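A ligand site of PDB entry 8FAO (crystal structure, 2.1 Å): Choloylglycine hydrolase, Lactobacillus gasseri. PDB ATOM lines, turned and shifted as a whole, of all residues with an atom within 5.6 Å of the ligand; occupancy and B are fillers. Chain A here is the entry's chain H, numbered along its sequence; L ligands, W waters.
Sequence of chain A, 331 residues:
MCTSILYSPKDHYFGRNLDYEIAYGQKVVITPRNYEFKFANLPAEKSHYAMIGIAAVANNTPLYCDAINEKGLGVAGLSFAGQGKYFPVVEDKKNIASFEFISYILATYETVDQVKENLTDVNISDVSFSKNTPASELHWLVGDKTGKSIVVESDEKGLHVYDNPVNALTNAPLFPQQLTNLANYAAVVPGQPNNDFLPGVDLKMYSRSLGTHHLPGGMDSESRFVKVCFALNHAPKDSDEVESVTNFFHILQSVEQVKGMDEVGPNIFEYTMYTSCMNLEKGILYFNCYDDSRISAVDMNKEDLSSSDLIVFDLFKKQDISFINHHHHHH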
ATOM      1  N   CYS A   2      20.909 -20.123   3.158  1.00  0.00           N
ATOM      2  CA  CYS A   2      21.747 -21.294   2.908  1.00  0.00           C
ATOM      3  C   CYS A   2      20.901 -22.571   2.968  1.00  0.00           C
ATOM      4  O   CYS A   2      21.335 -23.617   2.514  1.00  0.00           O
ATOM      5  CB  CYS A   2      22.876 -21.369   3.908  1.00  0.00           C
ATOM      6  SG  CYS A   2      24.278 -20.303   3.589  1.00  0.00           S
ATOM      7  N   THR A   3      19.734 -22.440   3.589  1.00  0.00           N
ATOM      8  CA  THR A   3      18.669 -23.435   3.572  1.00  0.00           C
ATOM      9  C   THR A   3      17.328 -22.805   3.258  1.00  0.00           C
ATOM     10  O   THR A   3      16.892 -21.871   3.940  1.00  0.00           O
ATOM     11  CB  THR A   3      18.596 -24.107   4.942  1.00  0.00           C
ATOM     12  OG1 THR A   3      19.942 -24.352   5.405  1.00  0.00           O
ATOM     13  CG2 THR A   3      17.809 -25.422   4.892  1.00  0.00           C
ATOM     14  N   ARG A  16      13.627 -19.164   4.150  1.00  0.00           N
ATOM     15  CA  ARG A  16      15.019 -19.573   4.136  1.00  0.00           C
ATOM     16  C   ARG A  16      15.759 -18.994   5.336  1.00  0.00           C
ATOM     17  O   ARG A  16      15.386 -17.938   5.871  1.00  0.00           O
ATOM     18  CB  ARG A  16      15.722 -19.135   2.849  1.00  0.00           C
ATOM     19  CG  ARG A  16      15.705 -17.623   2.617  1.00  0.00           C
ATOM     20  CD  ARG A  16      17.019 -16.962   3.064  1.00  0.00           C
ATOM     21  NE  ARG A  16      18.192 -17.524   2.381  1.00  0.00           N
ATOM     22  CZ  ARG A  16      18.596 -17.150   1.171  1.00  0.00           C
ATOM     23  NH1 ARG A  16      17.908 -16.291   0.428  1.00  0.00           N
ATOM     24  NH2 ARG A  16      19.736 -17.652   0.697  1.00  0.00           N
ATOM     25  N   ASN A  17      16.793 -19.708   5.765  1.00  0.00           N
ATOM     26  CA  ASN A  17      17.859 -19.133   6.566  1.00  0.00           C
ATOM     27  C   ASN A  17      18.803 -18.446   5.618  1.00  0.00           C
ATOM     28  O   ASN A  17      19.020 -18.922   4.508  1.00  0.00           O
ATOM     29  CB  ASN A  17      18.658 -20.195   7.323  1.00  0.00           C
ATOM     30  CG  ASN A  17      17.958 -20.735   8.555  1.00  0.00           C
ATOM     31  OD1 ASN A  17      17.153 -20.053   9.177  1.00  0.00           O
ATOM     32  ND2 ASN A  17      18.294 -21.958   8.918  1.00  0.00           N
ATOM     33  N   LEU A  18      19.405 -17.345   6.043  1.00  0.00           N
ATOM     34  CA  LEU A  18      20.504 -16.774   5.270  1.00  0.00           C
ATOM     35  C   LEU A  18      21.730 -16.780   6.170  1.00  0.00           C
ATOM     36  O   LEU A  18      21.786 -16.052   7.166  1.00  0.00           O
ATOM     37  CB  LEU A  18      20.195 -15.369   4.753  1.00  0.00           C
ATOM     38  CG  LEU A  18      21.205 -15.079   3.635  1.00  0.00           C
ATOM     39  CD1 LEU A  18      20.569 -14.407   2.454  1.00  0.00           C
ATOM     40  CD2 LEU A  18      22.343 -14.263   4.174  1.00  0.00           C
ATOM     41  N   ASP A  19      22.698 -17.625   5.819  1.00  0.00           N
ATOM     42  CA  ASP A  19      23.918 -17.828   6.587  1.00  0.00           C
ATOM     43  C   ASP A  19      25.085 -17.248   5.804  1.00  0.00           C
ATOM     44  O   ASP A  19      25.303 -17.613   4.648  1.00  0.00           O
ATOM     45  CB  ASP A  19      24.180 -19.329   6.871  1.00  0.00           C
ATOM     46  CG  ASP A  19      22.943 -20.099   7.354  1.00  0.00           C
ATOM     47  OD1 ASP A  19      22.085 -19.528   8.045  1.00  0.00           O
ATOM     48  OD2 ASP A  19      22.848 -21.316   7.076  1.00  0.00           O
ATOM     49  N   TYR A  20      25.842 -16.346   6.422  1.00  0.00           N
ATOM     50  CA  TYR A  20      27.003 -15.788   5.736  1.00  0.00           C
ATOM     51  C   TYR A  20      27.841 -15.041   6.768  1.00  0.00           C
ATOM     52  O   TYR A  20      27.444 -14.909   7.930  1.00  0.00           O
ATOM     53  CB  TYR A  20      26.599 -14.863   4.579  1.00  0.00           C
ATOM     54  CG  TYR A  20      27.560 -14.898   3.408  1.00  0.00           C
ATOM     55  CD1 TYR A  20      27.905 -16.097   2.799  1.00  0.00           C
ATOM     56  CD2 TYR A  20      28.127 -13.722   2.923  1.00  0.00           C
ATOM     57  CE1 TYR A  20      28.793 -16.126   1.731  1.00  0.00           C
ATOM     58  CE2 TYR A  20      29.018 -13.738   1.858  1.00  0.00           C
ATOM     59  CZ  TYR A  20      29.347 -14.936   1.267  1.00  0.00           C
ATOM     60  OH  TYR A  20      30.227 -14.935   0.203  1.00  0.00           O
ATOM     61  N   TYR A  24      24.577  -7.670   3.427  1.00  0.00           N
ATOM     62  CA  TYR A  24      24.507  -6.817   2.259  1.00  0.00           C
ATOM     63  C   TYR A  24      23.424  -5.759   2.413  1.00  0.00           C
ATOM     64  O   TYR A  24      22.724  -5.427   1.461  1.00  0.00           O
ATOM     65  CB  TYR A  24      24.249  -7.655   1.009  1.00  0.00           C
ATOM     66  CG  TYR A  24      25.397  -8.527   0.625  1.00  0.00           C
ATOM     67  CD1 TYR A  24      25.638  -9.735   1.284  1.00  0.00           C
ATOM     68  CD2 TYR A  24      26.243  -8.157  -0.400  1.00  0.00           C
ATOM     69  CE1 TYR A  24      26.711 -10.537   0.931  1.00  0.00           C
ATOM     70  CE2 TYR A  24      27.304  -8.954  -0.764  1.00  0.00           C
ATOM     71  CZ  TYR A  24      27.534 -10.146  -0.104  1.00  0.00           C
ATOM     72  OH  TYR A  24      28.595 -10.918  -0.484  1.00  0.00           O
ATOM     73  N   GLN A  26      20.521  -5.963   3.805  1.00  0.00           N
ATOM     74  CA  GLN A  26      19.218  -6.493   3.440  1.00  0.00           C
ATOM     75  C   GLN A  26      18.100  -5.784   4.221  1.00  0.00           C
ATOM     76  O   GLN A  26      18.263  -5.379   5.378  1.00  0.00           O
ATOM     77  CB  GLN A  26      19.167  -8.001   3.695  1.00  0.00           C
ATOM     78  CG  GLN A  26      19.925  -8.815   2.662  1.00  0.00           C
ATOM     79  CD  GLN A  26      21.290  -9.275   3.157  1.00  0.00           C
ATOM     80  OE1 GLN A  26      21.969  -8.563   3.911  1.00  0.00           O
ATOM     81  NE2 GLN A  26      21.710 -10.463   2.731  1.00  0.00           N
ATOM     82  N   ALA A  56      18.611  -6.513  -0.909  1.00  0.00           N
ATOM     83  CA  ALA A  56      19.473  -5.352  -0.873  1.00  0.00           C
ATOM     84  C   ALA A  56      18.908  -4.339  -1.863  1.00  0.00           C
ATOM     85  O   ALA A  56      18.464  -4.702  -2.945  1.00  0.00           O
ATOM     86  CB  ALA A  56      20.904  -5.723  -1.242  1.00  0.00           C
ATOM     87  N   LEU A  63      17.442  -5.878  -5.140  1.00  0.00           N
ATOM     88  CA  LEU A  63      18.242  -7.057  -5.468  1.00  0.00           C
ATOM     89  C   LEU A  63      17.829  -8.134  -4.472  1.00  0.00           C
ATOM     90  O   LEU A  63      18.379  -8.250  -3.385  1.00  0.00           O
ATOM     91  CB  LEU A  63      19.739  -6.726  -5.433  1.00  0.00           C
ATOM     92  CG  LEU A  63      20.215  -5.668  -6.445  1.00  0.00           C
ATOM     93  CD1 LEU A  63      21.615  -5.181  -6.125  1.00  0.00           C
ATOM     94  CD2 LEU A  63      20.184  -6.221  -7.851  1.00  0.00           C
ATOM     95  N   TYR A  64      16.816  -8.917  -4.849  1.00  0.00           N
ATOM     96  CA  TYR A  64      16.204  -9.843  -3.916  1.00  0.00           C
ATOM     97  C   TYR A  64      17.104 -11.047  -3.625  1.00  0.00           C
ATOM     98  O   TYR A  64      17.800 -11.542  -4.508  1.00  0.00           O
ATOM     99  CB  TYR A  64      14.871 -10.319  -4.481  1.00  0.00           C
ATOM    100  CG  TYR A  64      13.707  -9.394  -4.172  1.00  0.00           C
ATOM    101  CD1 TYR A  64      13.252  -9.237  -2.861  1.00  0.00           C
ATOM    102  CD2 TYR A  64      13.063  -8.691  -5.176  1.00  0.00           C
ATOM    103  CE1 TYR A  64      12.176  -8.409  -2.577  1.00  0.00           C
ATOM    104  CE2 TYR A  64      12.008  -7.837  -4.895  1.00  0.00           C
ATOM    105  CZ  TYR A  64      11.569  -7.706  -3.586  1.00  0.00           C
ATOM    106  OH  TYR A  64      10.511  -6.866  -3.308  1.00  0.00           O
ATOM    107  N   CYS A  65      17.114 -11.470  -2.362  1.00  0.00           N
ATOM    108  CA  CYS A  65      17.645 -12.774  -1.946  1.00  0.00           C
ATOM    109  C   CYS A  65      16.593 -13.864  -1.853  1.00  0.00           C
ATOM    110  O   CYS A  65      16.908 -15.034  -2.116  1.00  0.00           O
ATOM    111  CB  CYS A  65      18.344 -12.683  -0.587  1.00  0.00           C
ATOM    112  SG  CYS A  65      19.287 -11.189  -0.330  1.00  0.00           S
ATOM    113  N   GLY A  77      17.219 -17.387  -3.709  1.00  0.00           N
ATOM    114  CA  GLY A  77      18.531 -17.546  -4.306  1.00  0.00           C
ATOM    115  C   GLY A  77      19.557 -17.938  -3.252  1.00  0.00           C
ATOM    116  O   GLY A  77      19.683 -17.276  -2.216  1.00  0.00           O
ATOM    117  N   LEU A  78      20.279 -19.028  -3.526  1.00  0.00           N
ATOM    118  CA  LEU A  78      21.264 -19.546  -2.586  1.00  0.00           C
ATOM    119  C   LEU A  78      22.609 -19.654  -3.264  1.00  0.00           C
ATOM    120  O   LEU A  78      22.708 -19.950  -4.455  1.00  0.00           O
ATOM    121  CB  LEU A  78      20.866 -20.938  -2.041  1.00  0.00           C
ATOM    122  CG  LEU A  78      19.526 -21.032  -1.300  1.00  0.00           C
ATOM    123  CD1 LEU A  78      18.385 -21.286  -2.288  1.00  0.00           C
ATOM    124  CD2 LEU A  78      19.587 -22.155  -0.264  1.00  0.00           C
ATOM    125  N   SER A  79      23.655 -19.447  -2.478  1.00  0.00           N
ATOM    126  CA  SER A  79      25.021 -19.506  -3.004  1.00  0.00           C
ATOM    127  C   SER A  79      25.256 -20.853  -3.678  1.00  0.00           C
ATOM    128  O   SER A  79      24.855 -21.901  -3.165  1.00  0.00           O
ATOM    129  CB  SER A  79      26.023 -19.290  -1.865  1.00  0.00           C
ATOM    130  OG  SER A  79      27.320 -19.561  -2.348  1.00  0.00           O
ATOM    131  N   SER A  98      21.654 -13.122 -13.601  1.00  0.00           N
ATOM    132  CA  SER A  98      21.478 -13.841 -12.342  1.00  0.00           C
ATOM    133  C   SER A  98      20.913 -12.932 -11.252  1.00  0.00           C
ATOM    134  O   SER A  98      19.986 -13.319 -10.534  1.00  0.00           O
ATOM    135  CB  SER A  98      22.787 -14.497 -11.912  1.00  0.00           C
ATOM    136  OG  SER A  98      23.810 -13.572 -11.605  1.00  0.00           O
ATOM    137  N   PHE A  99      21.410 -11.686 -11.155  1.00  0.00           N
ATOM    138  CA  PHE A  99      20.943 -10.783 -10.115  1.00  0.00           C
ATOM    139  C   PHE A  99      19.472 -10.401 -10.277  1.00  0.00           C
ATOM    140  O   PHE A  99      18.847  -9.948  -9.321  1.00  0.00           O
ATOM    141  CB  PHE A  99      21.803  -9.504 -10.082  1.00  0.00           C
ATOM    142  CG  PHE A  99      21.679  -8.633 -11.324  1.00  0.00           C
ATOM    143  CD1 PHE A  99      22.515  -8.824 -12.411  1.00  0.00           C
ATOM    144  CD2 PHE A  99      20.726  -7.631 -11.397  1.00  0.00           C
ATOM    145  CE1 PHE A  99      22.401  -8.024 -13.551  1.00  0.00           C
ATOM    146  CE2 PHE A  99      20.607  -6.823 -12.536  1.00  0.00           C
ATOM    147  CZ  PHE A  99      21.447  -7.024 -13.614  1.00  0.00           C
ATOM    148  N   PHE A 129      25.090  -6.516 -12.197  1.00  0.00           N
ATOM    149  CA  PHE A 129      24.236  -5.368 -11.921  1.00  0.00           C
ATOM    150  C   PHE A 129      24.984  -4.062 -12.111  1.00  0.00           C
ATOM    151  O   PHE A 129      24.391  -3.067 -12.568  1.00  0.00           O
ATOM    152  CB  PHE A 129      23.691  -5.490 -10.498  1.00  0.00           C
ATOM    153  CG  PHE A 129      23.018  -4.241 -10.013  1.00  0.00           C
ATOM    154  CD1 PHE A 129      21.739  -3.921 -10.446  1.00  0.00           C
ATOM    155  CD2 PHE A 129      23.653  -3.388  -9.122  1.00  0.00           C
ATOM    156  CE1 PHE A 129      21.093  -2.758 -10.011  1.00  0.00           C
ATOM    157  CE2 PHE A 129      23.020  -2.230  -8.675  1.00  0.00           C
ATOM    158  CZ  PHE A 129      21.739  -1.922  -9.121  1.00  0.00           C
ATOM    159  N   THR A 133      29.346  -4.247  -8.245  1.00  0.00           N
ATOM    160  CA  THR A 133      28.714  -5.476  -7.755  1.00  0.00           C
ATOM    161  C   THR A 133      28.771  -6.554  -8.829  1.00  0.00           C
ATOM    162  O   THR A 133      27.817  -6.764  -9.585  1.00  0.00           O
ATOM    163  CB  THR A 133      27.265  -5.216  -7.312  1.00  0.00           C
ATOM    164  OG1 THR A 133      26.438  -5.058  -8.457  1.00  0.00           O
ATOM    165  CG2 THR A 133      27.171  -3.969  -6.452  1.00  0.00           C
ATOM    166  N   PRO A 134      29.883  -7.278  -8.911  1.00  0.00           N
ATOM    167  CA  PRO A 134      29.943  -8.437  -9.814  1.00  0.00           C
ATOM    168  C   PRO A 134      28.968  -9.525  -9.355  1.00  0.00           C
ATOM    169  O   PRO A 134      28.699  -9.670  -8.157  1.00  0.00           O
ATOM    170  CB  PRO A 134      31.400  -8.895  -9.704  1.00  0.00           C
ATOM    171  CG  PRO A 134      31.869  -8.367  -8.371  1.00  0.00           C
ATOM    172  CD  PRO A 134      31.126  -7.075  -8.143  1.00  0.00           C
ATOM    173  N   ALA A 135      28.453 -10.298 -10.311  1.00  0.00           N
ATOM    174  CA  ALA A 135      27.420 -11.294 -10.019  1.00  0.00           C
ATOM    175  C   ALA A 135      27.977 -12.421  -9.168  1.00  0.00           C
ATOM    176  O   ALA A 135      29.027 -12.991  -9.470  1.00  0.00           O
ATOM    177  CB  ALA A 135      26.863 -11.868 -11.309  1.00  0.00           C
ATOM    178  N   SER A 136      27.255 -12.773  -8.105  1.00  0.00           N
ATOM    179  CA  SER A 136      27.603 -13.935  -7.294  1.00  0.00           C
ATOM    180  C   SER A 136      26.989 -15.211  -7.887  1.00  0.00           C
ATOM    181  O   SER A 136      25.979 -15.175  -8.594  1.00  0.00           O
ATOM    182  CB  SER A 136      27.146 -13.741  -5.856  1.00  0.00           C
ATOM    183  OG  SER A 136      25.780 -13.365  -5.814  1.00  0.00           O
ATOM    184  N   LEU A 138      24.788 -18.337  -7.920  1.00  0.00           N
ATOM    185  CA  LEU A 138      23.551 -18.658  -7.230  1.00  0.00           C
ATOM    186  C   LEU A 138      22.865 -19.818  -7.937  1.00  0.00           C
ATOM    187  O   LEU A 138      23.071 -20.057  -9.127  1.00  0.00           O
ATOM    188  CB  LEU A 138      22.589 -17.469  -7.185  1.00  0.00           C
ATOM    189  CG  LEU A 138      23.008 -16.172  -6.470  1.00  0.00           C
ATOM    190  CD1 LEU A 138      21.961 -15.101  -6.696  1.00  0.00           C
ATOM    191  CD2 LEU A 138      23.175 -16.379  -4.994  1.00  0.00           C
ATOM    192  N   ASN A 171      23.311 -25.648  -0.674  1.00  0.00           N
ATOM    193  CA  ASN A 171      24.350 -25.119  -1.552  1.00  0.00           C
ATOM    194  C   ASN A 171      24.864 -26.238  -2.455  1.00  0.00           C
ATOM    195  O   ASN A 171      24.031 -26.993  -2.979  1.00  0.00           O
ATOM    196  CB  ASN A 171      25.405 -24.437  -0.675  1.00  0.00           C
ATOM    197  CG  ASN A 171      24.825 -23.359   0.214  1.00  0.00           C
ATOM    198  OD1 ASN A 171      24.876 -23.432   1.440  1.00  0.00           O
ATOM    199  ND2 ASN A 171      24.223 -22.369  -0.418  1.00  0.00           N
ATOM    200  N   GLU A 270      30.557 -17.975   9.339  1.00  0.00           N
ATOM    201  CA  GLU A 270      29.269 -17.964   8.666  1.00  0.00           C
ATOM    202  C   GLU A 270      28.229 -18.339   9.719  1.00  0.00           C
ATOM    203  O   GLU A 270      28.363 -19.390  10.367  1.00  0.00           O
ATOM    204  CB  GLU A 270      29.250 -18.941   7.486  1.00  0.00           C
ATOM    205  CG  GLU A 270      27.859 -19.387   7.000  1.00  0.00           C
ATOM    206  CD  GLU A 270      27.887 -20.084   5.621  1.00  0.00           C
ATOM    207  OE1 GLU A 270      28.485 -19.533   4.674  1.00  0.00           O
ATOM    208  OE2 GLU A 270      27.302 -21.193   5.483  1.00  0.00           O
HETATM  209  C1  LIG L   1      24.055 -16.637  -0.103  1.00  0.00           C
HETATM  210  C2  LIG L   1      22.495  -9.528  -5.495  1.00  0.00           C
HETATM  211  C3  LIG L   1      24.190 -15.110  -0.019  1.00  0.00           C
HETATM  212  C4  LIG L   1      25.645 -14.704   0.275  1.00  0.00           C
HETATM  213  C5  LIG L   1      22.398 -11.517  -3.310  1.00  0.00           C
HETATM  214  C6  LIG L   1      23.638 -14.528  -1.335  1.00  0.00           C
HETATM  215  C7  LIG L   1      22.156 -14.931  -1.571  1.00  0.00           C
HETATM  216  C8  LIG L   1      21.520 -13.840  -2.447  1.00  0.00           C
HETATM  217  C9  LIG L   1      22.688 -12.920  -2.815  1.00  0.00           C
HETATM  218  C10 LIG L   1      21.381 -11.516  -4.449  1.00  0.00           C
HETATM  219  C11 LIG L   1      21.163 -10.120  -5.028  1.00  0.00           C
HETATM  220  C12 LIG L   1      24.682 -17.375   1.088  1.00  0.00           C
HETATM  221  C13 LIG L   1      23.543 -18.983   2.612  1.00  0.00           C
HETATM  222  C14 LIG L   1      23.039 -10.288  -6.698  1.00  0.00           C
HETATM  223  C15 LIG L   1      24.300  -9.653  -7.239  1.00  0.00           C
HETATM  224  C16 LIG L   1      25.357  -9.565  -6.153  1.00  0.00           C
HETATM  225  C17 LIG L   1      24.830  -8.845  -4.912  1.00  0.00           C
HETATM  226  C18 LIG L   1      23.519  -9.431  -4.340  1.00  0.00           C
HETATM  227  C19 LIG L   1      24.070 -18.735   1.246  1.00  0.00           C
HETATM  228  C20 LIG L   1      23.010  -8.450  -3.273  1.00  0.00           C
HETATM  229  C21 LIG L   1      23.729 -10.856  -3.746  1.00  0.00           C
HETATM  230  C22 LIG L   1      24.747 -10.916  -2.605  1.00  0.00           C
HETATM  231  C23 LIG L   1      24.961 -12.326  -2.019  1.00  0.00           C
HETATM  232  C24 LIG L   1      23.631 -12.985  -1.592  1.00  0.00           C
HETATM  233  C25 LIG L   1      23.073 -12.272  -0.356  1.00  0.00           C
HETATM  234  O1  LIG L   1      23.958 -19.540   0.343  1.00  0.00           O
HETATM  235  O2  LIG L   1      24.797 -10.450  -8.331  1.00  0.00           O
HETATM  236  O3  LIG L   1      25.554 -13.101  -3.066  1.00  0.00           O
HETATM  237  O   HOH W   1      28.464 -13.071  -2.325  1.00  0.00           O
HETATM  238  O   HOH W   2      25.552  -8.473 -10.144  1.00  0.00           O
HETATM  239  O   HOH W   3      24.187 -12.999  -8.822  1.00  0.00           O
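Water W3 lies within hydrogen-bond range of an oxygen (O2) of the ligand (2.7 Å), the backbone carbonyl oxygen of Ser 136 (2.8 Å) and the side-chain hydroxyl of Ser 98 (2.9 Å). Water W2 lies within hydrogen-bond range of O2 of the ligand (2.8 Å), N of Phe 129 (2.9 Å), O of Thr 133 (2.9 Å) and N of Ala 135 (3.4 Å). Water W1 bridges OH of Tyr 24 and O3 of the ligand.
Merely in contact with the ligand: Asp 19 (3.0 Å), Tyr 20 (3.7 Å), Tyr 24 (3.7 Å), Gln 26 (3.8 Å), Ala 56 (3.9996 Å), Leu 63 (3.7 Å), Tyr 64 (3.6 Å), Cys 65 (3.9 Å), Gly 77 (3.5 Å), Leu 78 (3.9 Å), Phe 99 (3.6 Å), Pro 134 (3.9 Å), Ala 135 (3.2 Å) and Leu 138 (3.9 Å). Hydrophobic or aromatic side chains within 4 Å of the ligand: Tyr 20, Tyr 24, Ala 56, Leu 63, Phe 99, Ala 135 and Leu 138. The nearest printed residue that does not touch the ligand is Arg 16 (4.3 Å).
The side-chain sulfur (SG) of Cys 2 is bonded to a carbon (C13) of the ligand, at 1.8 Å. N of Ser 136 lies within hydrogen-bond range of O2 of the ligand, at 3.4 Å. The side-chain hydroxyl (OG) of Ser 136 is in hydrogen-bond range of an oxygen (O3) of the ligand (2.8 Å). The backbone NH (N) of Ser 79 is in hydrogen-bond range of an oxygen (O1) of the ligand (2.8 Å). The side-chain amide nitrogen of Asn 171 lies within hydrogen-bond range of an oxygen (O1) of the ligand (2.9 Å).
The backbone carbonyl oxygen (O) of Asn 17 lies within hydrogen-bond range of the backbone NH (N) of Cys 2 (2.6 Å). The backbone carbonyl oxygen (O) of Ser 79 is in hydrogen-bond range of the side-chain amide nitrogen (ND2) of Asn 171 (2.9 Å). The backbone carbonyl oxygen of Cys 65 sits at hydrogen-bond distance from the backbone NH of Gly 77, at 2.9 Å. The guanidinium group of Arg 16 is in hydrogen-bond range of the backbone carbonyl oxygen of Gly 77 (2.9 Å). N of Leu 63 sits at hydrogen-bond distance from O of Ala 56, at 2.7 Å. N of Tyr 24 is in hydrogen-bond range of OE1 of Gln 26 (2.8 Å). NH1 of Arg 16 sits at hydrogen-bond distance from O of Cys 65, 3.0 Å away.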
